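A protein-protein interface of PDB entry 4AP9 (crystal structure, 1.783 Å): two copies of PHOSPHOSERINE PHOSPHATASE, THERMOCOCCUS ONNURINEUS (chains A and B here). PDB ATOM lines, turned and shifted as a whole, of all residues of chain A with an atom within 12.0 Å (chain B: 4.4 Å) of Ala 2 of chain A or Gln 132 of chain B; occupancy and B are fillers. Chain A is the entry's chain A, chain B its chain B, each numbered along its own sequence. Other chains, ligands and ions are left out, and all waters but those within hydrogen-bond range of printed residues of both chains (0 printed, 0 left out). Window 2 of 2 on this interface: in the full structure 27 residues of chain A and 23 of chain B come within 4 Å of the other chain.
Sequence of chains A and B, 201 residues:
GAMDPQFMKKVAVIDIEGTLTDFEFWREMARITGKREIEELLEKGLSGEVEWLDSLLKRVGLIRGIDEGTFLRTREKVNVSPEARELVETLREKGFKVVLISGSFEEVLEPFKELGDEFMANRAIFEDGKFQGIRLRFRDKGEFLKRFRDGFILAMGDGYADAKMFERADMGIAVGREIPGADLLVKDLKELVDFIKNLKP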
ATOM      1  N   GLY A   1      20.844  22.919 -19.031  1.00  0.00           N
ATOM      2  CA  GLY A   1      20.895  23.265 -20.439  1.00  0.00           C
ATOM      3  C   GLY A   1      20.156  22.255 -21.298  1.00  0.00           C
ATOM      4  O   GLY A   1      20.768  21.535 -22.090  1.00  0.00           O
ATOM      5  N   ALA A   2      18.833  22.218 -21.157  1.00  0.00           N
ATOM      6  CA  ALA A   2      18.024  21.197 -21.809  1.00  0.00           C
ATOM      7  C   ALA A   2      17.425  21.672 -23.126  1.00  0.00           C
ATOM      8  O   ALA A   2      16.397  21.135 -23.584  1.00  0.00           O
ATOM      9  CB  ALA A   2      16.919  20.702 -20.855  1.00  0.00           C
ATOM     10  N   MET A   3      18.048  22.678 -23.744  1.00  0.00           N
ATOM     11  CA  MET A   3      17.513  23.148 -25.019  1.00  0.00           C
ATOM     12  C   MET A   3      18.430  24.036 -25.879  1.00  0.00           C
ATOM     13  O   MET A   3      18.913  25.077 -25.444  1.00  0.00           O
ATOM     14  CB  MET A   3      16.143  23.783 -24.798  1.00  0.00           C
ATOM     15  CG  MET A   3      15.276  23.725 -26.004  1.00  0.00           C
ATOM     16  SD  MET A   3      15.559  25.275 -27.110  1.00  0.00           S
ATOM     17  CE  MET A   3      14.081  26.343 -26.394  1.00  0.00           C
ATOM     18  N   ASP A   4      18.664  23.586 -27.108  1.00  0.00           N
ATOM     19  CA  ASP A   4      19.464  24.309 -28.094  1.00  0.00           C
ATOM     20  C   ASP A   4      18.500  24.800 -29.170  1.00  0.00           C
ATOM     21  O   ASP A   4      17.969  24.006 -29.934  1.00  0.00           O
ATOM     22  CB  ASP A   4      20.508  23.359 -28.698  1.00  0.00           C
ATOM     23  CG  ASP A   4      21.365  24.018 -29.768  1.00  0.00           C
ATOM     24  OD1 ASP A   4      21.132  25.203 -30.088  1.00  0.00           O
ATOM     25  OD2 ASP A   4      22.273  23.331 -30.292  1.00  0.00           O
ATOM     26  N   PRO A   5      18.246  26.114 -29.215  1.00  0.00           N
ATOM     27  CA  PRO A   5      17.286  26.657 -30.179  1.00  0.00           C
ATOM     28  C   PRO A   5      17.923  26.820 -31.560  1.00  0.00           C
ATOM     29  O   PRO A   5      17.971  27.932 -32.096  1.00  0.00           O
ATOM     30  CB  PRO A   5      16.957  28.029 -29.590  1.00  0.00           C
ATOM     31  CG  PRO A   5      18.261  28.438 -28.909  1.00  0.00           C
ATOM     32  CD  PRO A   5      18.911  27.171 -28.422  1.00  0.00           C
ATOM     33  N   GLN A   6      18.377  25.710 -32.135  1.00  0.00           N
ATOM     34  CA  GLN A   6      19.196  25.730 -33.350  1.00  0.00           C
ATOM     35  C   GLN A   6      18.519  26.442 -34.512  1.00  0.00           C
ATOM     36  O   GLN A   6      19.187  27.097 -35.320  1.00  0.00           O
ATOM     37  CB  GLN A   6      19.550  24.302 -33.765  1.00  0.00           C
ATOM     38  CG  GLN A   6      20.518  24.207 -34.931  1.00  0.00           C
ATOM     39  CD  GLN A   6      20.671  22.786 -35.422  1.00  0.00           C
ATOM     40  OE1 GLN A   6      20.335  22.471 -36.564  1.00  0.00           O
ATOM     41  NE2 GLN A   6      21.167  21.912 -34.551  1.00  0.00           N
ATOM     42  N   PHE A   7      17.203  26.293 -34.621  1.00  0.00           N
ATOM     43  CA  PHE A   7      16.497  26.870 -35.759  1.00  0.00           C
ATOM     44  C   PHE A   7      16.604  28.392 -35.800  1.00  0.00           C
ATOM     45  O   PHE A   7      16.439  28.996 -36.858  1.00  0.00           O
ATOM     46  CB  PHE A   7      15.037  26.409 -35.843  1.00  0.00           C
ATOM     47  CG  PHE A   7      14.133  27.019 -34.825  1.00  0.00           C
ATOM     48  CD1 PHE A   7      14.002  26.448 -33.573  1.00  0.00           C
ATOM     49  CD2 PHE A   7      13.376  28.133 -35.132  1.00  0.00           C
ATOM     50  CE1 PHE A   7      13.145  26.998 -32.625  1.00  0.00           C
ATOM     51  CE2 PHE A   7      12.515  28.692 -34.182  1.00  0.00           C
ATOM     52  CZ  PHE A   7      12.402  28.123 -32.939  1.00  0.00           C
ATOM     53  N   LYS A   9      19.354  30.189 -35.024  1.00  0.00           N
ATOM     54  CA  LYS A   9      20.737  30.660 -35.100  1.00  0.00           C
ATOM     55  C   LYS A   9      21.146  31.163 -36.483  1.00  0.00           C
ATOM     56  O   LYS A   9      20.680  30.654 -37.497  1.00  0.00           O
ATOM     57  CB  LYS A   9      21.699  29.553 -34.671  1.00  0.00           C
ATOM     58  CG  LYS A   9      21.538  29.125 -33.219  1.00  0.00           C
ATOM     59  CD  LYS A   9      22.740  28.331 -32.733  1.00  0.00           C
ATOM     60  CE  LYS A   9      22.286  27.063 -32.024  1.00  0.00           C
ATOM     61  NZ  LYS A   9      23.253  26.641 -30.978  1.00  0.00           N
ATOM     62  N   VAL B  60      10.717  16.734 -22.095  1.00  0.00           N
ATOM     63  CA  VAL B  60      12.180  16.746 -22.069  1.00  0.00           C
ATOM     64  C   VAL B  60      12.694  16.872 -20.632  1.00  0.00           C
ATOM     65  O   VAL B  60      13.603  16.154 -20.208  1.00  0.00           O
ATOM     66  CB  VAL B  60      12.755  17.878 -22.950  1.00  0.00           C
ATOM     67  CG1 VAL B  60      14.244  18.062 -22.683  1.00  0.00           C
ATOM     68  CG2 VAL B  60      12.496  17.589 -24.423  1.00  0.00           C
ATOM     69  N   ARG B  64      15.347  14.238 -18.387  1.00  0.00           N
ATOM     70  CA  ARG B  64      16.697  14.742 -18.190  1.00  0.00           C
ATOM     71  C   ARG B  64      17.422  13.823 -17.221  1.00  0.00           C
ATOM     72  O   ARG B  64      16.860  13.441 -16.205  1.00  0.00           O
ATOM     73  CB  ARG B  64      16.674  16.162 -17.643  1.00  0.00           C
ATOM     74  CG  ARG B  64      18.054  16.740 -17.379  1.00  0.00           C
ATOM     75  CD  ARG B  64      17.942  18.070 -16.663  1.00  0.00           C
ATOM     76  NE  ARG B  64      17.175  17.933 -15.428  1.00  0.00           N
ATOM     77  CZ  ARG B  64      17.712  17.904 -14.212  1.00  0.00           C
ATOM     78  NH1 ARG B  64      19.024  18.021 -14.064  1.00  0.00           N
ATOM     79  NH2 ARG B  64      16.934  17.770 -13.144  1.00  0.00           N
ATOM     80  N   ILE B 125      20.710  16.192 -26.859  1.00  0.00           N
ATOM     81  CA  ILE B 125      21.943  16.700 -26.265  1.00  0.00           C
ATOM     82  C   ILE B 125      22.351  15.725 -25.184  1.00  0.00           C
ATOM     83  O   ILE B 125      21.568  15.458 -24.271  1.00  0.00           O
ATOM     84  CB  ILE B 125      21.740  18.084 -25.628  1.00  0.00           C
ATOM     85  CG1 ILE B 125      21.170  19.069 -26.652  1.00  0.00           C
ATOM     86  CG2 ILE B 125      23.051  18.610 -25.040  1.00  0.00           C
ATOM     87  CD1 ILE B 125      20.701  20.375 -26.022  1.00  0.00           C
ATOM     88  N   GLU B 127      25.468  14.758 -22.346  1.00  0.00           N
ATOM     89  CA  GLU B 127      26.650  15.201 -21.623  1.00  0.00           C
ATOM     90  C   GLU B 127      27.004  14.149 -20.587  1.00  0.00           C
ATOM     91  O   GLU B 127      26.136  13.693 -19.852  1.00  0.00           O
ATOM     92  CB  GLU B 127      26.374  16.538 -20.938  1.00  0.00           C
ATOM     93  CG  GLU B 127      27.466  17.569 -21.128  1.00  0.00           C
ATOM     94  CD  GLU B 127      26.915  18.966 -21.372  1.00  0.00           C
ATOM     95  OE1 GLU B 127      25.733  19.085 -21.790  1.00  0.00           O
ATOM     96  OE2 GLU B 127      27.672  19.943 -21.146  1.00  0.00           O
ATOM     97  N   LYS B 130      24.626  11.150 -20.259  1.00  0.00           N
ATOM     98  CA  LYS B 130      23.229  11.329 -19.862  1.00  0.00           C
ATOM     99  C   LYS B 130      22.522  12.303 -20.809  1.00  0.00           C
ATOM    100  O   LYS B 130      23.145  13.235 -21.339  1.00  0.00           O
ATOM    101  CB  LYS B 130      23.126  11.852 -18.425  1.00  0.00           C
ATOM    102  CG  LYS B 130      23.903  11.036 -17.399  1.00  0.00           C
ATOM    103  CD  LYS B 130      23.499   9.570 -17.458  1.00  0.00           C
ATOM    104  CE  LYS B 130      24.488   8.675 -16.706  1.00  0.00           C
ATOM    105  NZ  LYS B 130      24.184   7.222 -16.897  1.00  0.00           N
ATOM    106  N   PHE B 131      21.226  12.081 -21.023  1.00  0.00           N
ATOM    107  CA  PHE B 131      20.408  12.993 -21.818  1.00  0.00           C
ATOM    108  C   PHE B 131      20.184  14.302 -21.069  1.00  0.00           C
ATOM    109  O   PHE B 131      19.750  14.308 -19.915  1.00  0.00           O
ATOM    110  CB  PHE B 131      19.055  12.350 -22.172  1.00  0.00           C
ATOM    111  CG  PHE B 131      18.097  13.287 -22.868  1.00  0.00           C
ATOM    112  CD1 PHE B 131      18.229  13.559 -24.223  1.00  0.00           C
ATOM    113  CD2 PHE B 131      17.079  13.905 -22.161  1.00  0.00           C
ATOM    114  CE1 PHE B 131      17.345  14.423 -24.861  1.00  0.00           C
ATOM    115  CE2 PHE B 131      16.201  14.765 -22.782  1.00  0.00           C
ATOM    116  CZ  PHE B 131      16.329  15.026 -24.138  1.00  0.00           C
ATOM    117  N   GLN B 132      20.471  15.412 -21.733  1.00  0.00           N
ATOM    118  CA  GLN B 132      20.340  16.717 -21.102  1.00  0.00           C
ATOM    119  C   GLN B 132      19.209  17.551 -21.676  1.00  0.00           C
ATOM    120  O   GLN B 132      18.624  18.364 -20.965  1.00  0.00           O
ATOM    121  CB  GLN B 132      21.657  17.490 -21.196  1.00  0.00           C
ATOM    122  CG  GLN B 132      22.801  16.796 -20.498  1.00  0.00           C
ATOM    123  CD  GLN B 132      22.481  16.483 -19.056  1.00  0.00           C
ATOM    124  OE1 GLN B 132      21.660  17.162 -18.425  1.00  0.00           O
ATOM    125  NE2 GLN B 132      23.125  15.451 -18.519  1.00  0.00           N
ATOM    126  N   GLY B 133      18.904  17.358 -22.955  1.00  0.00           N
ATOM    127  CA  GLY B 133      17.908  18.178 -23.610  1.00  0.00           C
ATOM    128  C   GLY B 133      17.805  18.001 -25.116  1.00  0.00           C
ATOM    129  O   GLY B 133      18.417  17.115 -25.708  1.00  0.00           O
ATOM    130  N   ILE B 134      17.019  18.875 -25.728  1.00  0.00           N
ATOM    131  CA  ILE B 134      16.657  18.761 -27.132  1.00  0.00           C
ATOM    132  C   ILE B 134      17.220  19.916 -27.964  1.00  0.00           C
ATOM    133  O   ILE B 134      17.264  21.060 -27.516  1.00  0.00           O
ATOM    134  CB  ILE B 134      15.127  18.724 -27.294  1.00  0.00           C
ATOM    135  CG1 ILE B 134      14.746  18.460 -28.750  1.00  0.00           C
ATOM    136  CG2 ILE B 134      14.509  20.029 -26.803  1.00  0.00           C
ATOM    137  CD1 ILE B 134      13.264  18.084 -28.953  1.00  0.00           C
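Ala 2 of chain A touches four residues of chain B. Of the printed residues of chain A, Gln 132 of chain B touches Gly 1 (3.99 Å) and Ala 2 (2.9 Å). Of chain A, only Ala 2 (3.9 Å) comes within 4 Å of Val 60 of chain B. No residue of chain A comes within 4 Å of Arg 64 of chain B. Printed residues of chain A within 4 Å of Ile 125 of chain B: Asp 4. No residue of chain A comes within 4 Å of Glu 127 of chain B. Of the printed residues of chain A, Gly 133 of chain B touches Ala 2 (3.3 Å). Of chain A, only Ala 2 (3.2 Å), Met 3 (3.3 Å) and Asp 4 (2.9 Å) come within 4 Å of Ile 134 of chain B. Printed residues of chain B within 4 Å of Gly 1 of chain A: Gln 132 (3.99 Å). Printed residues of chain B within 4 Å of Asp 4 of chain A: Ile 125 and Ile 134. Printed residues of chain B within 4 Å of Met 3 of chain A: Ile 134 (3.3 Å). Pro 5 of chain A touches none of the printed residues of chain B. The nearest printed residue of chain B that does not touch Ala 2 of chain A is Ile 125 of chain B (4.6 Å). The nearest printed residue of chain A that does not touch Gln 132 of chain B is Met 3 of chain A (5.2 Å). The nearest printed residue of chain B that does not touch Gly 1 of chain A is Ile 125 of chain B (4.1 Å).
N of Gln 6 of chain A lies close to OD1 of Asp 4 of chain A (3.5 Å). The side-chain carboxylate (OD1) of Asp 4 of chain A is in salt-bridge range of the side-chain amino group (NZ) of Lys 9 of chain A, 2.7 Å away. The backbone carbonyl oxygen of Ile 125 of chain B lies within hydrogen-bond range of the backbone NH of Gln 132 of chain B, 2.8 Å away. The backbone NH of Ile 125 of chain B lies within hydrogen-bond range of the backbone carbonyl oxygen of Gly 133 of chain B (2.7 Å).
Printed residues of chain A that touch a printed residue of chain B: Gly 1, Ala 2, Met 3 and Asp 4. Of the 9 printed residues of chain B, 5 touch a printed residue of chain A. Printed residues of chain B that touch a printed residue of chain A: Val 60, Ile 125, Gln 132, Gly 133 and Ile 134. Hydrophobic or aromatic side chains of chain B that line the printed part of chain A: Val 60, Ile 125 and Ile 134. Along chain B the printed residues that touch a printed residue of chain A span positions 60 to 134. Among the printed residues, 8 pairs touch across the chains.
No position is printed for both chains. Of the 8 pairs that touch across the chains among the printed residues, none has its exchanged pair printed and touching as well.
Gly 1 of chain A touches Gln 132 of chain B. Ala 2 of chain A touches Val 60 of chain B (O to CG1, 3.9 Å). O of Gln 132 of chain B touches CB of Ala 2 of chain A, 2.9 Å away. Ala 2 of chain A touches Gly 133 of chain B. Met 3 of chain A touches Ile 134 of chain B (CA to O, 3.3 Å). N of Asp 4 of chain A touches CD1 of Ile 125 of chain B (3.95 Å).
O of Ala 2 of chain A sits at hydrogen-bond distance from N of Ile 134 of chain B (3.2 Å). The backbone NH of Asp 4 of chain A lies within hydrogen-bond range of the backbone carbonyl oxygen of Ile 134 of chain B, at 2.9 Å.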
